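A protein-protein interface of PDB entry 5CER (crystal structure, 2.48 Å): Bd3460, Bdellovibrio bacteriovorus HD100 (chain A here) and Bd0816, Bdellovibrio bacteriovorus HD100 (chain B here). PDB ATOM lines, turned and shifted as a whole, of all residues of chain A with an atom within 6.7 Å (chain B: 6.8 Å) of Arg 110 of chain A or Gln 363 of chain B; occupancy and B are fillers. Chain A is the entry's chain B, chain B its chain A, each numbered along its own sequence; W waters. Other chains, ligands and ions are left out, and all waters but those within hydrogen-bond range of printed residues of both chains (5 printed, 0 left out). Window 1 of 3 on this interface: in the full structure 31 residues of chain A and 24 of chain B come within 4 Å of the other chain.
Of chain B, only Gly 359 and Gln 363 come within 4 Å of Arg 110 of chain A.
Ala 112 of chain A touches none of the printed residues of chain B.
Printed residues of chain A within 4 Å of Gln 363 of chain B: Arg 110 (3.2 Å), Gln 113 (3.4 Å) and Asn 114 (3.3 Å).
Met 364 of chain B touches none of the printed residues of chain A.
Of the printed residues of chain A, Asn 367 of chain B touches Gln 113 and Tyr 147.
Of the printed residues of chain A, Ser 370 of chain B touches Tyr 147.
The nearest residue of chain A that does not touch Gln 363 of chain B is Asp 105 of chain A (5.4 Å).
The side-chain amide nitrogen (ND2) of Asn 114 of chain A lies within hydrogen-bond range of the side-chain amide oxygen (OE1) of Gln 363 of chain B.
NZ of Lys 366 of chain B is in salt-bridge range of OD2 of Asp 80 of chain A (2.7 Å).
NE2 of Gln 363 of chain B is in hydrogen-bond range of OE1 of Gln 113 of chain A, at 3.4 Å.
OD1 of Asn 114 of chain A sits at hydrogen-bond distance from NZ of Lys 366 of chain B (3.2 Å).
The side-chain amide oxygen (OD1) of Asn 114 of chain A sits at hydrogen-bond distance from the backbone NH (N) of Gly 310 of chain B (3.0 Å).
The side-chain hydroxyl (OG) of Ser 370 of chain B lies within hydrogen-bond range of the backbone carbonyl oxygen (O) of Tyr 147 of chain A (3.0 Å).
Among the printed residues, merely in contact across the chains: Asn 79 of chain A with Arg 358 of chain B, Arg 110 of chain A with Gln 363 of chain B, Tyr 147 of chain A with Asn 367 of chain B, Gln 113 of chain A with Gly 310 of chain B, Gln 113 of chain A with Asn 367 of chain B, Asn 79 of chain A with Gly 359 of chain B, Thr 78 of chain A with Gly 359 of chain B and Arg 110 of chain A with Gly 359 of chain B.
Water W1 lies within hydrogen-bond range of OG of Ser 362 of chain B (2.6 Å), OD2 of Asp 80 of chain A (2.9 Å) and O of Thr 78 of chain A (3.1 Å).
Water W3 lies within hydrogen-bond range of NH1 of Arg 110 of chain A (2.8 Å), O of Gly 359 of chain B (2.8 Å) and O of Thr 78 of chain A (2.9 Å).
Water W2 bridges ND2 of Asn 79 of chain A (2.9 Å) and N of Gly 359 of chain B (2.9 Å).
Water W4 lies within hydrogen-bond range of the side-chain amide oxygen (OD1) of Asn 114 of chain A, the side-chain amide nitrogen (NE2) of Gln 363 of chain B and the backbone carbonyl oxygen (O) of Gly 310 of chain B.
Water W5 bridges the side-chain hydroxyl (OH) of Tyr 147 of chain A (3.0 Å) and the backbone carbonyl oxygen (O) of Asn 367 of chain B (3.3 Å).
The side-chain amide oxygen (OD1) of Asn 367 of chain B sits at hydrogen-bond distance from the side-chain amide nitrogen (NE2) of Gln 363 of chain B, 3.2 Å away.
O of Ala 74 of chain A sits at hydrogen-bond distance from OG1 of Thr 78 of chain A (2.7 Å).
OD2 of Asp 105 of chain A lies within salt-bridge range of NH2 of Arg 110 of chain A (2.8 Å).
ND2 of Asn 114 of chain A sits at hydrogen-bond distance from O of Arg 110 of chain A (2.9 Å).
OG of Ser 370 of chain B lies within hydrogen-bond range of O of Lys 366 of chain B (3.0 Å).
OG1 of Thr 78 of chain A sits at hydrogen-bond distance from ND2 of Asn 79 of chain A (3.4 Å).
Of the 13 printed residues of chain B, 7 touch a printed residue of chain A.
Among the printed residues, 14 pairs touch across the chains.
Among the printed residues, Asp or Glu carboxylates within 4 Å of a Lys or Arg side-chain nitrogen of the other chain: Asp 80 of chain A with Lys 366 of chain B (2.7 Å).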
ATOM      1  N   GLU A  70     -19.744   5.618  17.218  1.00  0.00           N
ATOM      2  CA  GLU A  70     -19.517   5.217  18.590  1.00  0.00           C
ATOM      3  C   GLU A  70     -19.216   3.723  18.754  1.00  0.00           C
ATOM      4  O   GLU A  70     -19.874   2.878  18.148  1.00  0.00           O
ATOM      5  CB  GLU A  70     -20.772   5.550  19.427  1.00  0.00           C
ATOM      6  CG  GLU A  70     -21.035   7.049  19.596  1.00  0.00           C
ATOM      7  CD  GLU A  70     -22.218   7.341  20.521  1.00  0.00           C
ATOM      8  OE1 GLU A  70     -23.273   6.694  20.336  1.00  0.00           O
ATOM      9  OE2 GLU A  70     -22.053   8.180  21.435  1.00  0.00           O
ATOM     10  N   ALA A  74     -18.229   3.778  24.138  1.00  0.00           N
ATOM     11  CA  ALA A  74     -18.910   5.049  24.038  1.00  0.00           C
ATOM     12  C   ALA A  74     -20.387   4.919  24.406  1.00  0.00           C
ATOM     13  O   ALA A  74     -20.946   5.829  25.085  1.00  0.00           O
ATOM     14  CB  ALA A  74     -18.742   5.675  22.632  1.00  0.00           C
ATOM     15  N   VAL A  77     -20.590   4.736  28.286  1.00  0.00           N
ATOM     16  CA  VAL A  77     -20.320   6.010  28.954  1.00  0.00           C
ATOM     17  C   VAL A  77     -21.470   6.954  28.750  1.00  0.00           C
ATOM     18  O   VAL A  77     -21.956   7.554  29.720  1.00  0.00           O
ATOM     19  CB  VAL A  77     -18.967   6.635  28.490  1.00  0.00           C
ATOM     20  CG1 VAL A  77     -18.828   8.093  28.901  1.00  0.00           C
ATOM     21  CG2 VAL A  77     -17.800   5.821  29.054  1.00  0.00           C
ATOM     22  N   THR A  78     -21.872   7.142  27.494  1.00  0.00           N
ATOM     23  CA  THR A  78     -22.910   8.132  27.166  1.00  0.00           C
ATOM     24  C   THR A  78     -24.247   7.796  27.814  1.00  0.00           C
ATOM     25  O   THR A  78     -25.034   8.686  28.109  1.00  0.00           O
ATOM     26  CB  THR A  78     -23.105   8.303  25.641  1.00  0.00           C
ATOM     27  OG1 THR A  78     -23.370   7.036  25.030  1.00  0.00           O
ATOM     28  CG2 THR A  78     -21.887   8.957  24.998  1.00  0.00           C
ATOM     29  N   ASN A  79     -24.507   6.515  28.047  1.00  0.00           N
ATOM     30  CA  ASN A  79     -25.754   6.059  28.714  1.00  0.00           C
ATOM     31  C   ASN A  79     -25.573   5.671  30.186  1.00  0.00           C
ATOM     32  O   ASN A  79     -26.401   4.979  30.754  1.00  0.00           O
ATOM     33  CB  ASN A  79     -26.358   4.916  27.918  1.00  0.00           C
ATOM     34  CG  ASN A  79     -26.857   5.365  26.571  1.00  0.00           C
ATOM     35  OD1 ASN A  79     -27.926   5.970  26.489  1.00  0.00           O
ATOM     36  ND2 ASN A  79     -26.093   5.134  25.511  1.00  0.00           N
ATOM     37  N   ASP A  80     -24.528   6.185  30.837  1.00  0.00           N
ATOM     38  CA  ASP A  80     -24.333   6.059  32.299  1.00  0.00           C
ATOM     39  C   ASP A  80     -24.215   4.635  32.859  1.00  0.00           C
ATOM     40  O   ASP A  80     -24.561   4.373  34.024  1.00  0.00           O
ATOM     41  CB  ASP A  80     -25.418   6.857  33.069  1.00  0.00           C
ATOM     42  CG  ASP A  80     -25.342   8.352  32.838  1.00  0.00           C
ATOM     43  OD1 ASP A  80     -24.252   8.916  32.507  1.00  0.00           O
ATOM     44  OD2 ASP A  80     -26.388   8.992  33.018  1.00  0.00           O
ATOM     45  N   TYR A  82     -21.625   2.883  33.793  1.00  0.00           N
ATOM     46  CA  TYR A  82     -20.192   2.998  34.125  1.00  0.00           C
ATOM     47  C   TYR A  82     -19.578   1.714  34.646  1.00  0.00           C
ATOM     48  O   TYR A  82     -18.398   1.483  34.451  1.00  0.00           O
ATOM     49  CB  TYR A  82     -19.944   4.168  35.058  1.00  0.00           C
ATOM     50  CG  TYR A  82     -19.954   5.466  34.308  1.00  0.00           C
ATOM     51  CD1 TYR A  82     -18.868   5.844  33.560  1.00  0.00           C
ATOM     52  CD2 TYR A  82     -21.095   6.312  34.324  1.00  0.00           C
ATOM     53  CE1 TYR A  82     -18.879   7.016  32.827  1.00  0.00           C
ATOM     54  CE2 TYR A  82     -21.116   7.494  33.616  1.00  0.00           C
ATOM     55  CZ  TYR A  82     -19.998   7.836  32.871  1.00  0.00           C
ATOM     56  OH  TYR A  82     -19.976   9.010  32.172  1.00  0.00           O
ATOM     57  N   VAL A  99     -17.251  10.563  21.432  1.00  0.00           N
ATOM     58  CA  VAL A  99     -18.657  10.213  21.560  1.00  0.00           C
ATOM     59  C   VAL A  99     -19.444  11.062  20.569  1.00  0.00           C
ATOM     60  O   VAL A  99     -18.947  12.095  20.102  1.00  0.00           O
ATOM     61  CB  VAL A  99     -19.190  10.400  23.002  1.00  0.00           C
ATOM     62  CG1 VAL A  99     -18.320   9.623  23.993  1.00  0.00           C
ATOM     63  CG2 VAL A  99     -19.307  11.868  23.421  1.00  0.00           C
ATOM     64  N   ALA A 100     -20.651  10.619  20.232  1.00  0.00           N
ATOM     65  CA  ALA A 100     -21.471  11.268  19.194  1.00  0.00           C
ATOM     66  C   ALA A 100     -21.921  12.678  19.629  1.00  0.00           C
ATOM     67  O   ALA A 100     -21.866  13.028  20.799  1.00  0.00           O
ATOM     68  CB  ALA A 100     -22.698  10.415  18.886  1.00  0.00           C
ATOM     69  N   GLY A 101     -22.399  13.435  18.657  1.00  0.00           N
ATOM     70  CA  GLY A 101     -22.880  14.792  18.869  1.00  0.00           C
ATOM     71  C   GLY A 101     -22.020  15.780  18.116  1.00  0.00           C
ATOM     72  O   GLY A 101     -20.920  15.431  17.650  1.00  0.00           O
ATOM     73  N   GLU A 103     -20.324  18.314  18.972  1.00  0.00           N
ATOM     74  CA  GLU A 103     -19.179  18.919  19.601  1.00  0.00           C
ATOM     75  C   GLU A 103     -17.895  18.086  19.417  1.00  0.00           C
ATOM     76  O   GLU A 103     -16.774  18.631  19.510  1.00  0.00           O
ATOM     77  CB  GLU A 103     -19.460  19.113  21.080  1.00  0.00           C
ATOM     78  CG  GLU A 103     -20.771  19.827  21.397  1.00  0.00           C
ATOM     79  CD  GLU A 103     -21.941  18.893  21.749  1.00  0.00           C
ATOM     80  OE1 GLU A 103     -21.922  17.669  21.527  1.00  0.00           O
ATOM     81  OE2 GLU A 103     -22.948  19.423  22.231  1.00  0.00           O
ATOM     82  N   ASP A 105     -17.068  15.634  21.555  1.00  0.00           N
ATOM     83  CA  ASP A 105     -16.566  15.440  22.911  1.00  0.00           C
ATOM     84  C   ASP A 105     -15.715  14.176  23.008  1.00  0.00           C
ATOM     85  O   ASP A 105     -16.074  13.137  22.415  1.00  0.00           O
ATOM     86  CB  ASP A 105     -17.743  15.304  23.905  1.00  0.00           C
ATOM     87  CG  ASP A 105     -18.394  16.646  24.280  1.00  0.00           C
ATOM     88  OD1 ASP A 105     -17.844  17.738  23.947  1.00  0.00           O
ATOM     89  OD2 ASP A 105     -19.433  16.575  24.964  1.00  0.00           O
ATOM     90  N   THR A 106     -14.618  14.235  23.777  1.00  0.00           N
ATOM     91  CA  THR A 106     -13.845  13.041  24.030  1.00  0.00           C
ATOM     92  C   THR A 106     -14.618  12.185  25.036  1.00  0.00           C
ATOM     93  O   THR A 106     -15.444  12.678  25.801  1.00  0.00           O
ATOM     94  CB  THR A 106     -12.460  13.338  24.591  1.00  0.00           C
ATOM     95  OG1 THR A 106     -12.564  13.961  25.859  1.00  0.00           O
ATOM     96  CG2 THR A 106     -11.679  14.235  23.641  1.00  0.00           C
ATOM     97  N   LEU A 107     -14.376  10.880  24.980  1.00  0.00           N
ATOM     98  CA  LEU A 107     -14.886   9.986  25.999  1.00  0.00           C
ATOM     99  C   LEU A 107     -14.549  10.485  27.405  1.00  0.00           C
ATOM    100  O   LEU A 107     -15.408  10.420  28.299  1.00  0.00           O
ATOM    101  CB  LEU A 107     -14.316   8.568  25.821  1.00  0.00           C
ATOM    102  CG  LEU A 107     -15.020   7.512  26.677  1.00  0.00           C
ATOM    103  CD1 LEU A 107     -16.365   7.110  26.065  1.00  0.00           C
ATOM    104  CD2 LEU A 107     -14.111   6.305  26.829  1.00  0.00           C
ATOM    105  N   PHE A 108     -13.304  10.954  27.593  1.00  0.00           N
ATOM    106  CA  PHE A 108     -12.859  11.453  28.902  1.00  0.00           C
ATOM    107  C   PHE A 108     -13.741  12.587  29.390  1.00  0.00           C
ATOM    108  O   PHE A 108     -14.153  12.630  30.563  1.00  0.00           O
ATOM    109  CB  PHE A 108     -11.399  11.925  28.879  1.00  0.00           C
ATOM    110  CG  PHE A 108     -11.027  12.659  30.122  1.00  0.00           C
ATOM    111  CD1 PHE A 108     -10.906  11.962  31.341  1.00  0.00           C
ATOM    112  CD2 PHE A 108     -10.919  14.061  30.128  1.00  0.00           C
ATOM    113  CE1 PHE A 108     -10.644  12.643  32.520  1.00  0.00           C
ATOM    114  CE2 PHE A 108     -10.649  14.747  31.307  1.00  0.00           C
ATOM    115  CZ  PHE A 108     -10.523  14.036  32.510  1.00  0.00           C
ATOM    116  N   MET A 109     -14.039  13.509  28.475  1.00  0.00           N
ATOM    117  CA  MET A 109     -14.958  14.635  28.763  1.00  0.00           C
ATOM    118  C   MET A 109     -16.324  14.164  29.298  1.00  0.00           C
ATOM    119  O   MET A 109     -16.834  14.720  30.267  1.00  0.00           O
ATOM    120  CB  MET A 109     -15.116  15.566  27.518  1.00  0.00           C
ATOM    121  CG  MET A 109     -13.909  16.484  27.299  1.00  0.00           C
ATOM    122  SD  MET A 109     -13.985  17.295  25.695  1.00  0.00           S
ATOM    123  CE  MET A 109     -15.211  18.578  26.016  1.00  0.00           C
ATOM    124  N   ARG A 110     -16.921  13.205  28.609  1.00  0.00           N
ATOM    125  CA  ARG A 110     -18.253  12.789  28.968  1.00  0.00           C
ATOM    126  C   ARG A 110     -18.198  12.105  30.357  1.00  0.00           C
ATOM    127  O   ARG A 110     -19.062  12.379  31.213  1.00  0.00           O
ATOM    128  CB  ARG A 110     -18.828  11.863  27.921  1.00  0.00           C
ATOM    129  CG  ARG A 110     -20.294  11.488  28.149  1.00  0.00           C
ATOM    130  CD  ARG A 110     -21.211  12.699  28.227  1.00  0.00           C
ATOM    131  NE  ARG A 110     -21.009  13.635  27.100  1.00  0.00           N
ATOM    132  CZ  ARG A 110     -21.594  13.556  25.910  1.00  0.00           C
ATOM    133  NH1 ARG A 110     -22.470  12.598  25.628  1.00  0.00           N
ATOM    134  NH2 ARG A 110     -21.331  14.472  24.999  1.00  0.00           N
ATOM    135  N   ALA A 111     -17.172  11.247  30.577  1.00  0.00           N
ATOM    136  CA  ALA A 111     -16.945  10.636  31.863  1.00  0.00           C
ATOM    137  C   ALA A 111     -16.638  11.665  32.969  1.00  0.00           C
ATOM    138  O   ALA A 111     -17.163  11.552  34.089  1.00  0.00           O
ATOM    139  CB  ALA A 111     -15.844   9.620  31.793  1.00  0.00           C
ATOM    140  N   ALA A 112     -15.835  12.678  32.665  1.00  0.00           N
ATOM    141  CA  ALA A 112     -15.491  13.693  33.650  1.00  0.00           C
ATOM    142  C   ALA A 112     -16.690  14.460  34.146  1.00  0.00           C
ATOM    143  O   ALA A 112     -16.728  14.840  35.313  1.00  0.00           O
ATOM    144  CB  ALA A 112     -14.468  14.656  33.078  1.00  0.00           C
ATOM    145  N   GLN A 113     -17.699  14.648  33.323  1.00  0.00           N
ATOM    146  CA  GLN A 113     -18.898  15.320  33.817  1.00  0.00           C
ATOM    147  C   GLN A 113     -19.738  14.466  34.757  1.00  0.00           C
ATOM    148  O   GLN A 113     -20.551  15.009  35.494  1.00  0.00           O
ATOM    149  CB  GLN A 113     -19.796  15.859  32.683  1.00  0.00           C
ATOM    150  CG  GLN A 113     -19.139  16.780  31.671  1.00  0.00           C
ATOM    151  CD  GLN A 113     -20.148  17.446  30.728  1.00  0.00           C
ATOM    152  OE1 GLN A 113     -20.234  17.118  29.534  1.00  0.00           O
ATOM    153  NE2 GLN A 113     -20.937  18.356  31.266  1.00  0.00           N
ATOM    154  N   ASN A 114     -19.584  13.154  34.729  1.00  0.00           N
ATOM    155  CA  ASN A 114     -20.600  12.256  35.274  1.00  0.00           C
ATOM    156  C   ASN A 114     -20.138  11.192  36.292  1.00  0.00           C
ATOM    157  O   ASN A 114     -20.927  10.840  37.190  1.00  0.00           O
ATOM    158  CB  ASN A 114     -21.316  11.593  34.067  1.00  0.00           C
ATOM    159  CG  ASN A 114     -22.197  12.573  33.318  1.00  0.00           C
ATOM    160  OD1 ASN A 114     -23.150  13.206  33.867  1.00  0.00           O
ATOM    161  ND2 ASN A 114     -21.848  12.758  32.060  1.00  0.00           N
ATOM    162  N   ASN A 115     -18.940  10.619  36.073  1.00  0.00           N
ATOM    163  CA  ASN A 115     -18.400   9.533  36.893  1.00  0.00           C
ATOM    164  C   ASN A 115     -16.899   9.666  37.087  1.00  0.00           C
ATOM    165  O   ASN A 115     -16.094   9.425  36.190  1.00  0.00           O
ATOM    166  CB  ASN A 115     -18.740   8.173  36.286  1.00  0.00           C
ATOM    167  CG  ASN A 115     -18.382   7.020  37.210  1.00  0.00           C
ATOM    168  OD1 ASN A 115     -17.226   6.564  37.277  1.00  0.00           O
ATOM    169  ND2 ASN A 115     -19.372   6.566  37.976  1.00  0.00           N
ATOM    170  N   ALA A 140     -12.674  19.100  29.113  1.00  0.00           N
ATOM    171  CA  ALA A 140     -13.498  18.828  30.268  1.00  0.00           C
ATOM    172  C   ALA A 140     -13.685  20.055  31.154  1.00  0.00           C
ATOM    173  O   ALA A 140     -14.795  20.305  31.659  1.00  0.00           O
ATOM    174  CB  ALA A 140     -12.906  17.677  31.076  1.00  0.00           C
ATOM    175  N   TYR A 147     -21.346  23.632  33.536  1.00  0.00           N
ATOM    176  CA  TYR A 147     -22.453  22.803  34.023  1.00  0.00           C
ATOM    177  C   TYR A 147     -22.162  21.944  35.235  1.00  0.00           C
ATOM    178  O   TYR A 147     -22.977  21.118  35.624  1.00  0.00           O
ATOM    179  CB  TYR A 147     -22.957  21.929  32.854  1.00  0.00           C
ATOM    180  CG  TYR A 147     -23.400  22.736  31.629  1.00  0.00           C
ATOM    181  CD1 TYR A 147     -24.302  23.803  31.761  1.00  0.00           C
ATOM    182  CD2 TYR A 147     -22.949  22.423  30.337  1.00  0.00           C
ATOM    183  CE1 TYR A 147     -24.726  24.539  30.652  1.00  0.00           C
ATOM    184  CE2 TYR A 147     -23.402  23.133  29.225  1.00  0.00           C
ATOM    185  CZ  TYR A 147     -24.270  24.209  29.396  1.00  0.00           C
ATOM    186  OH  TYR A 147     -24.671  24.970  28.354  1.00  0.00           O
ATOM    187  N   GLY B 310     -24.283  13.498  36.672  1.00  0.00           N
ATOM    188  CA  GLY B 310     -23.333  14.458  37.243  1.00  0.00           C
ATOM    189  C   GLY B 310     -23.727  15.887  36.955  1.00  0.00           C
ATOM    190  O   GLY B 310     -24.830  16.178  36.453  1.00  0.00           O
ATOM    191  N   ARG B 358     -29.844   8.390  21.846  1.00  0.00           N
ATOM    192  CA  ARG B 358     -30.135   8.310  23.287  1.00  0.00           C
ATOM    193  C   ARG B 358     -29.076   9.063  24.109  1.00  0.00           C
ATOM    194  O   ARG B 358     -29.409   9.863  24.957  1.00  0.00           O
ATOM    195  CB  ARG B 358     -30.220   6.860  23.753  1.00  0.00           C
ATOM    196  CG  ARG B 358     -30.952   6.706  25.081  1.00  0.00           C
ATOM    197  CD  ARG B 358     -30.791   5.319  25.629  1.00  0.00           C
ATOM    198  NE  ARG B 358     -31.609   4.351  24.927  1.00  0.00           N
ATOM    199  CZ  ARG B 358     -31.694   3.067  25.242  1.00  0.00           C
ATOM    200  NH1 ARG B 358     -30.978   2.550  26.234  1.00  0.00           N
ATOM    201  NH2 ARG B 358     -32.495   2.301  24.531  1.00  0.00           N
ATOM    202  N   GLY B 359     -27.804   8.806  23.819  1.00  0.00           N
ATOM    203  CA  GLY B 359     -26.681   9.463  24.511  1.00  0.00           C
ATOM    204  C   GLY B 359     -26.627  10.965  24.309  1.00  0.00           C
ATOM    205  O   GLY B 359     -26.311  11.705  25.233  1.00  0.00           O
ATOM    206  N   VAL B 360     -26.922  11.400  23.094  1.00  0.00           N
ATOM    207  CA  VAL B 360     -26.947  12.823  22.758  1.00  0.00           C
ATOM    208  C   VAL B 360     -28.062  13.515  23.555  1.00  0.00           C
ATOM    209  O   VAL B 360     -27.852  14.520  24.170  1.00  0.00           O
ATOM    210  CB  VAL B 360     -27.132  13.003  21.231  1.00  0.00           C
ATOM    211  CG1 VAL B 360     -27.406  14.449  20.868  1.00  0.00           C
ATOM    212  CG2 VAL B 360     -25.917  12.518  20.479  1.00  0.00           C
ATOM    213  N   ALA B 361     -29.247  12.920  23.561  1.00  0.00           N
ATOM    214  CA  ALA B 361     -30.373  13.451  24.293  1.00  0.00           C
ATOM    215  C   ALA B 361     -30.082  13.525  25.766  1.00  0.00           C
ATOM    216  O   ALA B 361     -30.418  14.524  26.414  1.00  0.00           O
ATOM    217  CB  ALA B 361     -31.625  12.622  24.051  1.00  0.00           C
ATOM    218  N   SER B 362     -29.470  12.475  26.309  1.00  0.00           N
ATOM    219  CA  SER B 362     -29.106  12.394  27.732  1.00  0.00           C
ATOM    220  C   SER B 362     -28.240  13.583  28.209  1.00  0.00           C
ATOM    221  O   SER B 362     -28.583  14.247  29.209  1.00  0.00           O
ATOM    222  CB  SER B 362     -28.396  11.033  27.981  1.00  0.00           C
ATOM    223  OG  SER B 362     -28.273  10.858  29.359  1.00  0.00           O
ATOM    224  N   GLN B 363     -27.165  13.913  27.478  1.00  0.00           N
ATOM    225  CA  GLN B 363     -26.296  15.017  27.867  1.00  0.00           C
ATOM    226  C   GLN B 363     -26.950  16.393  27.599  1.00  0.00           C
ATOM    227  O   GLN B 363     -26.658  17.367  28.325  1.00  0.00           O
ATOM    228  CB  GLN B 363     -24.933  14.908  27.224  1.00  0.00           C
ATOM    229  CG  GLN B 363     -23.851  15.730  27.936  1.00  0.00           C
ATOM    230  CD  GLN B 363     -23.620  15.298  29.377  1.00  0.00           C
ATOM    231  OE1 GLN B 363     -23.639  14.095  29.687  1.00  0.00           O
ATOM    232  NE2 GLN B 363     -23.453  16.270  30.277  1.00  0.00           N
ATOM    233  N   MET B 364     -27.841  16.492  26.610  1.00  0.00           N
ATOM    234  CA  MET B 364     -28.606  17.726  26.398  1.00  0.00           C
ATOM    235  C   MET B 364     -29.493  18.012  27.602  1.00  0.00           C
ATOM    236  O   MET B 364     -29.526  19.118  28.095  1.00  0.00           O
ATOM    237  CB  MET B 364     -29.476  17.648  25.149  1.00  0.00           C
ATOM    238  CG  MET B 364     -28.715  17.713  23.839  1.00  0.00           C
ATOM    239  SD  MET B 364     -29.781  17.533  22.370  1.00  0.00           S
ATOM    240  CE  MET B 364     -30.968  18.863  22.532  1.00  0.00           C
ATOM    241  N   ILE B 365     -30.184  16.996  28.095  1.00  0.00           N
ATOM    242  CA  ILE B 365     -31.054  17.147  29.253  1.00  0.00           C
ATOM    243  C   ILE B 365     -30.236  17.585  30.459  1.00  0.00           C
ATOM    244  O   ILE B 365     -30.629  18.493  31.192  1.00  0.00           O
ATOM    245  CB  ILE B 365     -31.846  15.847  29.540  1.00  0.00           C
ATOM    246  CG1 ILE B 365     -32.916  15.635  28.465  1.00  0.00           C
ATOM    247  CG2 ILE B 365     -32.505  15.892  30.906  1.00  0.00           C
ATOM    248  CD1 ILE B 365     -33.613  14.293  28.533  1.00  0.00           C
ATOM    249  N   LYS B 366     -29.100  16.936  30.658  1.00  0.00           N
ATOM    250  CA  LYS B 366     -28.239  17.244  31.817  1.00  0.00           C
ATOM    251  C   LYS B 366     -27.731  18.676  31.793  1.00  0.00           C
ATOM    252  O   LYS B 366     -27.681  19.349  32.840  1.00  0.00           O
ATOM    253  CB  LYS B 366     -27.049  16.264  31.905  1.00  0.00           C
ATOM    254  CG  LYS B 366     -27.467  14.870  32.353  1.00  0.00           C
ATOM    255  CD  LYS B 366     -26.314  13.910  32.201  1.00  0.00           C
ATOM    256  CE  LYS B 366     -26.758  12.494  32.563  1.00  0.00           C
ATOM    257  NZ  LYS B 366     -25.594  11.577  32.647  1.00  0.00           N
ATOM    258  N   ASN B 367     -27.332  19.115  30.613  1.00  0.00           N
ATOM    259  CA  ASN B 367     -26.862  20.468  30.460  1.00  0.00           C
ATOM    260  C   ASN B 367     -27.979  21.487  30.619  1.00  0.00           C
ATOM    261  O   ASN B 367     -27.759  22.568  31.164  1.00  0.00           O
ATOM    262  CB  ASN B 367     -26.125  20.625  29.128  1.00  0.00           C
ATOM    263  CG  ASN B 367     -24.803  19.867  29.087  1.00  0.00           C
ATOM    264  OD1 ASN B 367     -24.255  19.399  30.127  1.00  0.00           O
ATOM    265  ND2 ASN B 367     -24.257  19.777  27.912  1.00  0.00           N
ATOM    266  N   LYS B 368     -29.185  21.109  30.220  1.00  0.00           N
ATOM    267  CA  LYS B 368     -30.340  21.972  30.399  1.00  0.00           C
ATOM    268  C   LYS B 368     -30.641  22.156  31.857  1.00  0.00           C
ATOM    269  O   LYS B 368     -30.809  23.264  32.314  1.00  0.00           O
ATOM    270  CB  LYS B 368     -31.543  21.388  29.698  1.00  0.00           C
ATOM    271  CG  LYS B 368     -32.384  22.413  28.967  1.00  0.00           C
ATOM    272  CD  LYS B 368     -33.335  21.711  28.003  1.00  0.00           C
ATOM    273  CE  LYS B 368     -33.483  22.331  26.626  1.00  0.00           C
ATOM    274  NZ  LYS B 368     -32.474  23.293  26.164  1.00  0.00           N
ATOM    275  N   SER B 370     -28.466  21.754  34.362  1.00  0.00           N
ATOM    276  CA  SER B 370     -27.378  22.587  34.875  1.00  0.00           C
ATOM    277  C   SER B 370     -27.598  24.089  34.611  1.00  0.00           C
ATOM    278  O   SER B 370     -27.330  24.912  35.477  1.00  0.00           O
ATOM    279  CB  SER B 370     -26.036  22.135  34.328  1.00  0.00           C
ATOM    280  OG  SER B 370     -25.796  20.782  34.682  1.00  0.00           O
HETATM  281  O   HOH W   1     -27.251   8.629  30.324  1.00  0.00           O
HETATM  282  O   HOH W   2     -26.885   6.186  22.979  1.00  0.00           O
HETATM  283  O   HOH W   3     -24.349  11.308  27.170  1.00  0.00           O
HETATM  284  O   HOH W   4     -23.495  16.076  33.449  1.00  0.00           O
HETATM  285  O   HOH W   5     -27.645  24.837  28.779  1.00  0.00           O
